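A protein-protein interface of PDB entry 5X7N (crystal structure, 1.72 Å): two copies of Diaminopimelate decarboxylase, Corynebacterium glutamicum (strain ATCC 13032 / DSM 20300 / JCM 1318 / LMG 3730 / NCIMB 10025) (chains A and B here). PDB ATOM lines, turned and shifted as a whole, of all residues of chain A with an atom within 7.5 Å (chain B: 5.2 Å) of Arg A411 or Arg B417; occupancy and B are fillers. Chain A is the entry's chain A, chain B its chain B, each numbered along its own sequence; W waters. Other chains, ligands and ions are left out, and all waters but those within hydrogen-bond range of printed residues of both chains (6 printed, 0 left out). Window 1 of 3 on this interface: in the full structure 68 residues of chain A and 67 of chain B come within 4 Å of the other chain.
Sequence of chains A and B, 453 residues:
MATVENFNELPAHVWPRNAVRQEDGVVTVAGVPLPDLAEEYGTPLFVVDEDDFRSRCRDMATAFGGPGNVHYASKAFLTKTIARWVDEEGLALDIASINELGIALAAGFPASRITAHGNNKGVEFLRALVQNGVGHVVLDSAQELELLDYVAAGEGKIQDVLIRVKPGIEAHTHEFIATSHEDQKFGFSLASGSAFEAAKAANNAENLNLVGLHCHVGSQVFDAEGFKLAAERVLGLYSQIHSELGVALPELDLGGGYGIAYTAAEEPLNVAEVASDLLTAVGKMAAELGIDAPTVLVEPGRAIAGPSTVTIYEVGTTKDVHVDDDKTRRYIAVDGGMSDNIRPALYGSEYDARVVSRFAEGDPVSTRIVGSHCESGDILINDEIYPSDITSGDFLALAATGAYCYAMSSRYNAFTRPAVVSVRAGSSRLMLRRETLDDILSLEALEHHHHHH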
ATOM      1  N   ASN A  99     -24.302   8.326   5.349  1.00  0.00           N
ATOM      2  CA  ASN A  99     -24.783   9.508   6.009  1.00  0.00           C
ATOM      3  C   ASN A  99     -26.272   9.610   6.097  1.00  0.00           C
ATOM      4  O   ASN A  99     -26.772  10.152   7.115  1.00  0.00           O
ATOM      5  CB  ASN A  99     -24.146  10.789   5.401  1.00  0.00           C
ATOM      6  CG  ASN A  99     -22.606  10.926   5.671  1.00  0.00           C
ATOM      7  OD1 ASN A  99     -21.867  11.622   4.919  1.00  0.00           O
ATOM      8  ND2 ASN A  99     -22.117  10.245   6.680  1.00  0.00           N
ATOM      9  N   SER A 339     -28.279  27.497  -6.956  1.00  0.00           N
ATOM     10  CA  SER A 339     -27.745  26.947  -5.679  1.00  0.00           C
ATOM     11  C   SER A 339     -28.839  26.376  -4.742  1.00  0.00           C
ATOM     12  O   SER A 339     -28.497  25.590  -3.814  1.00  0.00           O
ATOM     13  CB  SER A 339     -27.008  27.993  -4.888  1.00  0.00           C
ATOM     14  OG  SER A 339     -27.801  29.223  -4.836  1.00  0.00           O
ATOM     15  N   ASP A 340     -30.103  26.786  -4.870  1.00  0.00           N
ATOM     16  CA  ASP A 340     -31.171  26.172  -4.050  1.00  0.00           C
ATOM     17  C   ASP A 340     -32.185  25.393  -4.864  1.00  0.00           C
ATOM     18  O   ASP A 340     -32.923  24.626  -4.287  1.00  0.00           O
ATOM     19  CB  ASP A 340     -31.893  27.197  -3.138  1.00  0.00           C
ATOM     20  CG  ASP A 340     -32.659  28.264  -3.918  1.00  0.00           C
ATOM     21  OD1 ASP A 340     -33.750  27.968  -4.428  1.00  0.00           O
ATOM     22  OD2 ASP A 340     -32.088  29.368  -4.073  1.00  0.00           O
ATOM     23  N   HIS A 373     -26.865  34.386  -9.331  1.00  0.00           N
ATOM     24  CA  HIS A 373     -25.534  33.867  -9.679  1.00  0.00           C
ATOM     25  C   HIS A 373     -24.973  34.444 -10.928  1.00  0.00           C
ATOM     26  O   HIS A 373     -25.682  34.844 -11.840  1.00  0.00           O
ATOM     27  CB  HIS A 373     -25.584  32.351  -9.833  1.00  0.00           C
ATOM     28  CG  HIS A 373     -25.868  31.664  -8.541  1.00  0.00           C
ATOM     29  ND1 HIS A 373     -24.912  31.524  -7.578  1.00  0.00           N
ATOM     30  CD2 HIS A 373     -26.984  31.101  -8.046  1.00  0.00           C
ATOM     31  CE1 HIS A 373     -25.426  30.932  -6.522  1.00  0.00           C
ATOM     32  NE2 HIS A 373     -26.686  30.661  -6.778  1.00  0.00           N
ATOM     33  N   MET A 408     -29.978  18.929  -3.358  1.00  0.00           N
ATOM     34  CA  MET A 408     -29.059  19.135  -4.424  1.00  0.00           C
ATOM     35  C   MET A 408     -28.478  20.544  -4.370  1.00  0.00           C
ATOM     36  O   MET A 408     -27.755  20.978  -5.280  1.00  0.00           O
ATOM     37  CB  MET A 408     -29.753  18.863  -5.806  1.00  0.00           C
ATOM     38  CG  MET A 408     -30.098  17.422  -5.991  1.00  0.00           C
ATOM     39  SD  MET A 408     -30.773  17.082  -7.637  1.00  0.00           S
ATOM     40  CE  MET A 408     -29.193  16.928  -8.342  1.00  0.00           C
ATOM     41  N   SER A 409     -28.738  21.243  -3.285  1.00  0.00           N
ATOM     42  CA  SER A 409     -28.241  22.608  -3.093  1.00  0.00           C
ATOM     43  C   SER A 409     -26.737  22.704  -2.982  1.00  0.00           C
ATOM     44  O   SER A 409     -26.093  21.757  -2.605  1.00  0.00           O
ATOM     45  CB  SER A 409     -28.837  23.243  -1.820  1.00  0.00           C
ATOM     46  OG  SER A 409     -28.480  22.522  -0.676  1.00  0.00           O
ATOM     47  N   SER A 410     -26.199  23.822  -3.479  1.00  0.00           N
ATOM     48  CA  SER A 410     -24.753  24.054  -3.562  1.00  0.00           C
ATOM     49  C   SER A 410     -24.417  25.385  -2.900  1.00  0.00           C
ATOM     50  O   SER A 410     -25.303  26.206  -2.579  1.00  0.00           O
ATOM     51  CB  SER A 410     -24.289  24.091  -5.014  1.00  0.00           C
ATOM     52  OG  SER A 410     -24.591  25.353  -5.647  1.00  0.00           O
ATOM     53  N   ARG A 411     -23.088  25.576  -2.707  1.00  0.00           N
ATOM     54  CA  ARG A 411     -22.564  26.866  -2.274  1.00  0.00           C
ATOM     55  C   ARG A 411     -21.887  27.582  -3.411  1.00  0.00           C
ATOM     56  O   ARG A 411     -20.898  28.261  -3.271  1.00  0.00           O
ATOM     57  CB  ARG A 411     -21.573  26.717  -1.085  1.00  0.00           C
ATOM     58  CG  ARG A 411     -22.164  26.119   0.187  1.00  0.00           C
ATOM     59  CD  ARG A 411     -21.040  25.759   1.143  1.00  0.00           C
ATOM     60  NE  ARG A 411     -21.575  25.418   2.444  1.00  0.00           N
ATOM     61  CZ  ARG A 411     -20.842  24.937   3.436  1.00  0.00           C
ATOM     62  NH1 ARG A 411     -19.493  24.812   3.260  1.00  0.00           N
ATOM     63  NH2 ARG A 411     -21.445  24.615   4.578  1.00  0.00           N
ATOM     64  N   TYR A 412     -22.483  27.475  -4.600  1.00  0.00           N
ATOM     65  CA  TYR A 412     -21.957  28.243  -5.744  1.00  0.00           C
ATOM     66  C   TYR A 412     -21.964  29.741  -5.463  1.00  0.00           C
ATOM     67  O   TYR A 412     -22.889  30.286  -4.825  1.00  0.00           O
ATOM     68  CB  TYR A 412     -22.723  27.869  -7.001  1.00  0.00           C
ATOM     69  CG  TYR A 412     -22.127  28.446  -8.281  1.00  0.00           C
ATOM     70  CD1 TYR A 412     -20.780  28.408  -8.488  1.00  0.00           C
ATOM     71  CD2 TYR A 412     -22.891  29.022  -9.230  1.00  0.00           C
ATOM     72  CE1 TYR A 412     -20.193  28.886  -9.659  1.00  0.00           C
ATOM     73  CE2 TYR A 412     -22.293  29.549 -10.419  1.00  0.00           C
ATOM     74  CZ  TYR A 412     -20.944  29.511 -10.583  1.00  0.00           C
ATOM     75  OH  TYR A 412     -20.324  30.003 -11.751  1.00  0.00           O
ATOM     76  N   ASN A 413     -20.871  30.428  -5.860  1.00  0.00           N
ATOM     77  CA  ASN A 413     -20.666  31.788  -5.467  1.00  0.00           C
ATOM     78  C   ASN A 413     -20.685  32.020  -3.933  1.00  0.00           C
ATOM     79  O   ASN A 413     -20.939  33.155  -3.498  1.00  0.00           O
ATOM     80  CB  ASN A 413     -21.662  32.739  -6.108  1.00  0.00           C
ATOM     81  CG  ASN A 413     -21.527  32.853  -7.613  1.00  0.00           C
ATOM     82  OD1 ASN A 413     -22.507  32.729  -8.344  1.00  0.00           O
ATOM     83  ND2 ASN A 413     -20.296  33.056  -8.086  1.00  0.00           N
ATOM     84  N   ALA A 414     -20.290  30.993  -3.169  1.00  0.00           N
ATOM     85  CA  ALA A 414     -20.335  30.977  -1.699  1.00  0.00           C
ATOM     86  C   ALA A 414     -21.712  31.328  -1.155  1.00  0.00           C
ATOM     87  O   ALA A 414     -21.800  31.912  -0.068  1.00  0.00           O
ATOM     88  CB  ALA A 414     -19.224  31.910  -1.128  1.00  0.00           C
ATOM     89  N   PHE A 415     -22.803  31.082  -1.881  1.00  0.00           N
ATOM     90  CA  PHE A 415     -24.133  31.261  -1.321  1.00  0.00           C
ATOM     91  C   PHE A 415     -24.323  30.222  -0.209  1.00  0.00           C
ATOM     92  O   PHE A 415     -23.803  29.098  -0.245  1.00  0.00           O
ATOM     93  CB  PHE A 415     -25.236  31.015  -2.352  1.00  0.00           C
ATOM     94  CG  PHE A 415     -25.480  32.180  -3.294  1.00  0.00           C
ATOM     95  CD1 PHE A 415     -24.485  33.061  -3.703  1.00  0.00           C
ATOM     96  CD2 PHE A 415     -26.756  32.359  -3.827  1.00  0.00           C
ATOM     97  CE1 PHE A 415     -24.778  34.125  -4.563  1.00  0.00           C
ATOM     98  CE2 PHE A 415     -27.029  33.403  -4.714  1.00  0.00           C
ATOM     99  CZ  PHE A 415     -26.036  34.224  -5.125  1.00  0.00           C
ATOM    100  N   THR A 416     -25.071  30.610   0.814  1.00  0.00           N
ATOM    101  CA  THR A 416     -25.337  29.807   1.954  1.00  0.00           C
ATOM    102  C   THR A 416     -26.622  29.011   1.702  1.00  0.00           C
ATOM    103  O   THR A 416     -27.565  29.561   1.149  1.00  0.00           O
ATOM    104  CB  THR A 416     -25.585  30.694   3.226  1.00  0.00           C
ATOM    105  OG1 THR A 416     -26.361  31.841   2.930  1.00  0.00           O
ATOM    106  CG2 THR A 416     -24.226  31.175   3.783  1.00  0.00           C
ATOM    107  N   ARG A 417     -26.649  27.755   2.135  1.00  0.00           N
ATOM    108  CA  ARG A 417     -27.914  26.944   2.085  1.00  0.00           C
ATOM    109  C   ARG A 417     -29.021  27.696   2.816  1.00  0.00           C
ATOM    110  O   ARG A 417     -28.777  28.201   3.932  1.00  0.00           O
ATOM    111  CB  ARG A 417     -27.766  25.534   2.665  1.00  0.00           C
ATOM    112  CG  ARG A 417     -27.206  24.579   1.632  1.00  0.00           C
ATOM    113  CD  ARG A 417     -26.875  23.198   2.096  1.00  0.00           C
ATOM    114  NE  ARG A 417     -26.091  22.605   0.970  1.00  0.00           N
ATOM    115  CZ  ARG A 417     -24.743  22.474   0.947  1.00  0.00           C
ATOM    116  NH1 ARG A 417     -24.124  21.943  -0.133  1.00  0.00           N
ATOM    117  NH2 ARG A 417     -23.991  22.765   2.073  1.00  0.00           N
ATOM    118  N   GLU A 435     -27.291  28.303   6.561  1.00  0.00           N
ATOM    119  CA  GLU A 435     -25.838  28.413   6.659  1.00  0.00           C
ATOM    120  C   GLU A 435     -25.367  29.829   6.774  1.00  0.00           C
ATOM    121  O   GLU A 435     -26.058  30.776   6.434  1.00  0.00           O
ATOM    122  CB  GLU A 435     -25.169  27.794   5.405  1.00  0.00           C
ATOM    123  CG  GLU A 435     -25.256  26.337   5.470  1.00  0.00           C
ATOM    124  CD  GLU A 435     -24.592  25.637   4.292  1.00  0.00           C
ATOM    125  OE1 GLU A 435     -24.419  26.305   3.222  1.00  0.00           O
ATOM    126  OE2 GLU A 435     -24.238  24.438   4.448  1.00  0.00           O
ATOM    127  N   THR A 436     -24.132  29.995   7.290  1.00  0.00           N
ATOM    128  CA  THR A 436     -23.538  31.323   7.441  1.00  0.00           C
ATOM    129  C   THR A 436     -22.159  31.320   6.730  1.00  0.00           C
ATOM    130  O   THR A 436     -21.607  30.271   6.430  1.00  0.00           O
ATOM    131  CB  THR A 436     -23.310  31.677   8.913  1.00  0.00           C
ATOM    132  OG1 THR A 436     -22.357  30.757   9.457  1.00  0.00           O
ATOM    133  CG2 THR A 436     -24.712  31.656   9.696  1.00  0.00           C
ATOM    134  N   LEU A 437     -21.626  32.514   6.631  1.00  0.00           N
ATOM    135  CA  LEU A 437     -20.199  32.660   6.177  1.00  0.00           C
ATOM    136  C   LEU A 437     -19.300  31.862   7.061  1.00  0.00           C
ATOM    137  O   LEU A 437     -18.318  31.288   6.605  1.00  0.00           O
ATOM    138  CB  LEU A 437     -19.803  34.129   6.144  1.00  0.00           C
ATOM    139  CG  LEU A 437     -18.353  34.409   5.684  1.00  0.00           C
ATOM    140  CD1 LEU A 437     -18.046  33.865   4.302  1.00  0.00           C
ATOM    141  CD2 LEU A 437     -18.023  35.866   5.770  1.00  0.00           C
ATOM    142  N   ASP A 438     -19.566  31.834   8.360  1.00  0.00           N
ATOM    143  CA  ASP A 438     -18.696  31.096   9.230  1.00  0.00           C
ATOM    144  C   ASP A 438     -18.682  29.594   8.910  1.00  0.00           C
ATOM    145  O   ASP A 438     -17.692  28.951   9.112  1.00  0.00           O
ATOM    146  CB  ASP A 438     -19.197  31.273  10.628  1.00  0.00           C
ATOM    147  CG  ASP A 438     -18.333  30.599  11.627  1.00  0.00           C
ATOM    148  OD1 ASP A 438     -17.230  31.181  11.898  1.00  0.00           O
ATOM    149  OD2 ASP A 438     -18.747  29.489  12.119  1.00  0.00           O
ATOM    150  N   ASP A 439     -19.823  29.039   8.533  1.00  0.00           N
ATOM    151  CA  ASP A 439     -19.873  27.642   8.079  1.00  0.00           C
ATOM    152  C   ASP A 439     -18.972  27.392   6.878  1.00  0.00           C
ATOM    153  O   ASP A 439     -18.246  26.449   6.847  1.00  0.00           O
ATOM    154  CB  ASP A 439     -21.303  27.272   7.663  1.00  0.00           C
ATOM    155  CG  ASP A 439     -22.277  27.244   8.821  1.00  0.00           C
ATOM    156  OD1 ASP A 439     -21.943  26.670   9.901  1.00  0.00           O
ATOM    157  OD2 ASP A 439     -23.408  27.767   8.670  1.00  0.00           O
ATOM    158  N   ILE A 440     -19.031  28.306   5.935  1.00  0.00           N
ATOM    159  CA  ILE A 440     -18.153  28.218   4.752  1.00  0.00           C
ATOM    160  C   ILE A 440     -16.699  28.300   5.124  1.00  0.00           C
ATOM    161  O   ILE A 440     -15.883  27.440   4.755  1.00  0.00           O
ATOM    162  CB  ILE A 440     -18.573  29.230   3.701  1.00  0.00           C
ATOM    163  CG1 ILE A 440     -19.944  28.804   3.210  1.00  0.00           C
ATOM    164  CG2 ILE A 440     -17.564  29.255   2.530  1.00  0.00           C
ATOM    165  CD1 ILE A 440     -20.588  29.756   2.254  1.00  0.00           C
ATOM    166  N   LEU A 441     -16.380  29.266   5.968  1.00  0.00           N
ATOM    167  CA  LEU A 441     -15.015  29.404   6.398  1.00  0.00           C
ATOM    168  C   LEU A 441     -14.505  28.334   7.366  1.00  0.00           C
ATOM    169  O   LEU A 441     -13.259  28.182   7.479  1.00  0.00           O
ATOM    170  CB  LEU A 441     -14.748  30.814   6.993  1.00  0.00           C
ATOM    171  CG  LEU A 441     -14.824  32.017   6.080  1.00  0.00           C
ATOM    172  CD1 LEU A 441     -14.833  33.334   6.809  1.00  0.00           C
ATOM    173  CD2 LEU A 441     -13.645  31.951   5.121  1.00  0.00           C
ATOM    174  N   SER A 442     -15.422  27.565   7.961  1.00  0.00           N
ATOM    175  CA  SER A 442     -15.095  26.551   8.949  1.00  0.00           C
ATOM    176  C   SER A 442     -14.259  25.447   8.320  1.00  0.00           C
ATOM    177  O   SER A 442     -13.431  24.810   9.007  1.00  0.00           O
ATOM    178  CB  SER A 442     -16.349  25.945   9.605  1.00  0.00           C
ATOM    179  OG  SER A 442     -17.057  25.065   8.778  1.00  0.00           O
ATOM    180  N   LEU A 443     -14.366  25.274   7.010  1.00  0.00           N
ATOM    181  CA  LEU A 443     -13.600  24.222   6.360  1.00  0.00           C
ATOM    182  C   LEU A 443     -12.139  24.546   6.102  1.00  0.00           C
ATOM    183  O   LEU A 443     -11.327  23.666   5.792  1.00  0.00           O
ATOM    184  CB  LEU A 443     -14.259  23.873   4.975  1.00  0.00           C
ATOM    185  CG  LEU A 443     -15.677  23.336   5.063  1.00  0.00           C
ATOM    186  CD1 LEU A 443     -16.131  23.042   3.645  1.00  0.00           C
ATOM    187  CD2 LEU A 443     -15.802  22.127   5.922  1.00  0.00           C
ATOM    188  N   TYR B 406     -15.629  21.991  -7.438  1.00  0.00           N
ATOM    189  CA  TYR B 406     -15.878  22.081  -5.992  1.00  0.00           C
ATOM    190  C   TYR B 406     -16.897  23.154  -5.672  1.00  0.00           C
ATOM    191  O   TYR B 406     -17.748  22.950  -4.811  1.00  0.00           O
ATOM    192  CB  TYR B 406     -14.541  22.422  -5.282  1.00  0.00           C
ATOM    193  CG  TYR B 406     -14.670  22.466  -3.791  1.00  0.00           C
ATOM    194  CD1 TYR B 406     -15.014  23.669  -3.185  1.00  0.00           C
ATOM    195  CD2 TYR B 406     -14.440  21.324  -3.005  1.00  0.00           C
ATOM    196  CE1 TYR B 406     -15.184  23.761  -1.827  1.00  0.00           C
ATOM    197  CE2 TYR B 406     -14.615  21.378  -1.636  1.00  0.00           C
ATOM    198  CZ  TYR B 406     -14.962  22.591  -1.033  1.00  0.00           C
ATOM    199  OH  TYR B 406     -15.141  22.597   0.359  1.00  0.00           O
ATOM    200  N   ALA B 407     -16.842  24.306  -6.330  1.00  0.00           N
ATOM    201  CA  ALA B 407     -17.807  25.387  -6.060  1.00  0.00           C
ATOM    202  C   ALA B 407     -19.250  24.970  -6.298  1.00  0.00           C
ATOM    203  O   ALA B 407     -20.167  25.441  -5.576  1.00  0.00           O
ATOM    204  CB  ALA B 407     -17.460  26.636  -6.933  1.00  0.00           C
ATOM    205  N   SER B 409     -20.388  21.863  -5.802  1.00  0.00           N
ATOM    206  CA  SER B 409     -20.578  20.593  -5.080  1.00  0.00           C
ATOM    207  C   SER B 409     -21.840  20.647  -4.219  1.00  0.00           C
ATOM    208  O   SER B 409     -22.325  21.738  -3.857  1.00  0.00           O
ATOM    209  CB  SER B 409     -19.391  20.230  -4.169  1.00  0.00           C
ATOM    210  OG  SER B 409     -19.123  21.219  -3.166  1.00  0.00           O
ATOM    211  N   ARG B 411     -24.484  18.210  -1.321  1.00  0.00           N
ATOM    212  CA  ARG B 411     -24.605  17.100  -0.355  1.00  0.00           C
ATOM    213  C   ARG B 411     -25.743  16.166  -0.754  1.00  0.00           C
ATOM    214  O   ARG B 411     -26.520  15.680   0.082  1.00  0.00           O
ATOM    215  CB  ARG B 411     -24.821  17.645   1.055  1.00  0.00           C
ATOM    216  CG  ARG B 411     -23.624  18.405   1.626  1.00  0.00           C
ATOM    217  CD  ARG B 411     -24.110  19.128   2.868  1.00  0.00           C
ATOM    218  NE  ARG B 411     -23.030  19.776   3.603  1.00  0.00           N
ATOM    219  CZ  ARG B 411     -23.254  20.596   4.630  1.00  0.00           C
ATOM    220  NH1 ARG B 411     -24.495  20.805   5.040  1.00  0.00           N
ATOM    221  NH2 ARG B 411     -22.213  21.153   5.261  1.00  0.00           N
ATOM    222  N   PHE B 415     -23.939  13.175   0.912  1.00  0.00           N
ATOM    223  CA  PHE B 415     -22.507  13.039   0.688  1.00  0.00           C
ATOM    224  C   PHE B 415     -21.799  14.291   1.239  1.00  0.00           C
ATOM    225  O   PHE B 415     -22.335  15.416   1.239  1.00  0.00           O
ATOM    226  CB  PHE B 415     -22.134  12.877  -0.790  1.00  0.00           C
ATOM    227  CG  PHE B 415     -22.288  11.515  -1.335  1.00  0.00           C
ATOM    228  CD1 PHE B 415     -23.308  10.619  -0.990  1.00  0.00           C
ATOM    229  CD2 PHE B 415     -21.491  11.148  -2.425  1.00  0.00           C
ATOM    230  CE1 PHE B 415     -23.436   9.424  -1.600  1.00  0.00           C
ATOM    231  CE2 PHE B 415     -21.606   9.913  -2.994  1.00  0.00           C
ATOM    232  CZ  PHE B 415     -22.600   9.071  -2.646  1.00  0.00           C
ATOM    233  N   THR B 416     -20.626  14.048   1.829  1.00  0.00           N
ATOM    234  CA  THR B 416     -19.825  15.093   2.424  1.00  0.00           C
ATOM    235  C   THR B 416     -18.929  15.745   1.353  1.00  0.00           C
ATOM    236  O   THR B 416     -18.438  15.066   0.504  1.00  0.00           O
ATOM    237  CB  THR B 416     -18.896  14.553   3.502  1.00  0.00           C
ATOM    238  OG1 THR B 416     -18.312  13.293   3.142  1.00  0.00           O
ATOM    239  CG2 THR B 416     -19.698  14.367   4.834  1.00  0.00           C
ATOM    240  N   ARG B 417     -18.779  17.033   1.420  1.00  0.00           N
ATOM    241  CA  ARG B 417     -17.836  17.685   0.480  1.00  0.00           C
ATOM    242  C   ARG B 417     -16.431  17.114   0.659  1.00  0.00           C
ATOM    243  O   ARG B 417     -15.911  16.996   1.784  1.00  0.00           O
ATOM    244  CB  ARG B 417     -17.748  19.182   0.704  1.00  0.00           C
ATOM    245  CG  ARG B 417     -18.509  20.093  -0.192  1.00  0.00           C
ATOM    246  CD  ARG B 417     -18.191  21.534   0.213  1.00  0.00           C
ATOM    247  NE  ARG B 417     -18.334  22.477  -0.863  1.00  0.00           N
ATOM    248  CZ  ARG B 417     -18.131  23.815  -0.800  1.00  0.00           C
ATOM    249  NH1 ARG B 417     -18.417  24.521  -1.932  1.00  0.00           N
ATOM    250  NH2 ARG B 417     -17.689  24.441   0.373  1.00  0.00           N
ATOM    251  N   PRO B 418     -15.730  16.879  -0.471  1.00  0.00           N
ATOM    252  CA  PRO B 418     -14.394  16.340  -0.397  1.00  0.00           C
ATOM    253  C   PRO B 418     -13.381  17.285   0.155  1.00  0.00           C
ATOM    254  O   PRO B 418     -13.536  18.488   0.083  1.00  0.00           O
ATOM    255  CB  PRO B 418     -14.040  16.074  -1.868  1.00  0.00           C
ATOM    256  CG  PRO B 418     -15.361  15.872  -2.485  1.00  0.00           C
ATOM    257  CD  PRO B 418     -16.277  16.837  -1.825  1.00  0.00           C
ATOM    258  N   ALA B 419     -12.303  16.714   0.713  1.00  0.00           N
ATOM    259  CA  ALA B 419     -11.148  17.556   1.102  1.00  0.00           C
ATOM    260  C   ALA B 419     -10.475  18.123  -0.148  1.00  0.00           C
ATOM    261  O   ALA B 419     -10.559  17.535  -1.240  1.00  0.00           O
ATOM    262  CB  ALA B 419     -10.112  16.755   1.857  1.00  0.00           C
ATOM    263  N   ARG B 433     -10.779  21.045   4.750  1.00  0.00           N
ATOM    264  CA  ARG B 433     -10.968  19.715   5.269  1.00  0.00           C
ATOM    265  C   ARG B 433     -12.232  19.103   4.616  1.00  0.00           C
ATOM    266  O   ARG B 433     -13.085  19.811   4.114  1.00  0.00           O
ATOM    267  CB  ARG B 433     -11.162  19.734   6.792  1.00  0.00           C
ATOM    268  CG  ARG B 433     -12.351  20.538   7.328  1.00  0.00           C
ATOM    269  CD  ARG B 433     -12.670  20.173   8.807  1.00  0.00           C
ATOM    270  NE  ARG B 433     -13.760  20.965   9.362  1.00  0.00           N
ATOM    271  CZ  ARG B 433     -15.051  20.598   9.272  1.00  0.00           C
ATOM    272  NH1 ARG B 433     -15.392  19.529   8.565  1.00  0.00           N
ATOM    273  NH2 ARG B 433     -15.979  21.332   9.781  1.00  0.00           N
ATOM    274  N   ARG B 434     -12.283  17.821   4.600  1.00  0.00           N
ATOM    275  CA  ARG B 434     -13.500  17.059   4.240  1.00  0.00           C
ATOM    276  C   ARG B 434     -14.631  17.402   5.223  1.00  0.00           C
ATOM    277  O   ARG B 434     -14.408  17.546   6.449  1.00  0.00           O
ATOM    278  CB  ARG B 434     -13.212  15.584   4.274  1.00  0.00           C
ATOM    279  CG  ARG B 434     -14.284  14.669   3.610  1.00  0.00           C
ATOM    280  CD  ARG B 434     -13.904  13.203   3.589  1.00  0.00           C
ATOM    281  NE  ARG B 434     -12.624  12.986   2.938  1.00  0.00           N
ATOM    282  CZ  ARG B 434     -12.411  13.014   1.631  1.00  0.00           C
ATOM    283  NH1 ARG B 434     -13.409  13.126   0.773  1.00  0.00           N
ATOM    284  NH2 ARG B 434     -11.162  13.036   1.172  1.00  0.00           N
ATOM    285  N   GLU B 435     -15.853  17.559   4.694  1.00  0.00           N
ATOM    286  CA  GLU B 435     -16.969  17.600   5.584  1.00  0.00           C
ATOM    287  C   GLU B 435     -17.176  16.266   6.286  1.00  0.00           C
ATOM    288  O   GLU B 435     -16.709  15.203   5.894  1.00  0.00           O
ATOM    289  CB  GLU B 435     -18.257  18.015   4.840  1.00  0.00           C
ATOM    290  CG  GLU B 435     -18.253  19.451   4.371  1.00  0.00           C
ATOM    291  CD  GLU B 435     -19.527  19.887   3.619  1.00  0.00           C
ATOM    292  OE1 GLU B 435     -20.207  18.964   3.116  1.00  0.00           O
ATOM    293  OE2 GLU B 435     -19.863  21.103   3.598  1.00  0.00           O
HETATM  294  O   HOH W   1     -19.184  23.016   5.550  1.00  0.00           O
HETATM  295  O   HOH W   2     -26.885  19.656  -1.053  1.00  0.00           O
HETATM  296  O   HOH W   3     -20.918  24.007  -3.403  1.00  0.00           O
HETATM  297  O   HOH W   4     -18.945  10.939   4.873  1.00  0.00           O
HETATM  298  O   HOH W   5     -14.427  23.197  11.354  1.00  0.00           O
HETATM  299  O   HOH W   6     -23.595  23.061   6.773  1.00  0.00           O
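N of Ser A410 lies within hydrogen-bond range of O of Ser A339 (2.9 Å).
The backbone carbonyl oxygen (O) of Asp A439 lies within hydrogen-bond range of the side-chain hydroxyl (OG) of Ser A442.
Water W3 lies within hydrogen-bond range of O of Ser B409 (2.7 Å), O of Ala B407 (2.7 Å), N of Arg A411 (2.8 Å) and NH1 of Arg B417 (2.9 Å).
Water W2 bridges the backbone carbonyl oxygen of Ser A409 (2.7 Å) and the backbone NH of Arg B411 (2.8 Å).
Arg A411 touches just these residues of chain B: Ala B407, Arg B411, Arg B417 and Glu B435.
Arg B417 touches just these residues of chain A: Arg A411 and Leu A443.
Printed residues of chain B within 4 Å of Tyr A412: Ala B407 (3.2 Å).
Printed residues of chain B within 4 Å of Ser A410: Ser B409.
Ile A440 touches none of the printed residues of chain B.
Asn A413 touches none of the printed residues of chain B.
The nearest printed residue of chain A that does not touch Tyr B406 is Arg A411 (5.7 Å).
Hydrophobic or aromatic side chains of chain B within 4 Å of the printed part of chain A: Tyr B406.
Of the 23 printed residues of chain A, 9 touch a printed residue of chain B.
Printed residues of chain A that touch a printed residue of chain B: Asn A99, Ser A409, Ser A410, Arg A411, Tyr A412, Arg A417, Glu A435, Ser A442 and Leu A443.
Hydrophobic or aromatic side chains of chain A within 4 Å of the printed part of chain B: Tyr A412 and Leu A443.
Among the printed residues, Asp or Glu carboxylates within 4 Å of a Lys or Arg side-chain nitrogen of the other chain: Arg A411 with Glu B435 and Glu A435 with Arg B411.
Ser A409 touches its own counterpart, Ser B409.
Arg B411 touches its own counterpart, Arg A411.
Arg A411 touches Arg B417, and with the chains exchanged Arg A417 touches Arg B411.
Arg A411 touches Glu B435, and with the chains exchanged Glu A435 touches Arg B411.
The guanidinium group of Arg A411 sits close to the guanidinium group of Arg B417 (3.4 Å).
The backbone NH of Tyr A412 sits at hydrogen-bond distance from the backbone carbonyl oxygen of Ala B407 (3.2 Å).
The guanidinium group (NH1) of Arg B411 lies within salt-bridge range of the side-chain carboxylate (OE2) of Glu A435 (3.7 Å).
The guanidinium group (NE) of Arg B411 sits close to the guanidinium group (NH2) of Arg A417.
The backbone carbonyl oxygen of Leu A443 sits at hydrogen-bond distance from the backbone NH of Arg B433, at 2.9 Å.
The guanidinium group of Arg A411 lies within salt-bridge range of the side-chain carboxylate of Glu B435.
Among the printed residues, merely in contact across the chains: Ser A410 with Ser B409, Leu A443 with Tyr B406, Arg A411 with Ala B407, Asn A99 with Thr B416, Arg A411 with Arg B411, Ser A442 with Arg B433, Leu A443 with Arg B417, Leu A443 with Glu B435 and Ser A409 with Ser B409.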
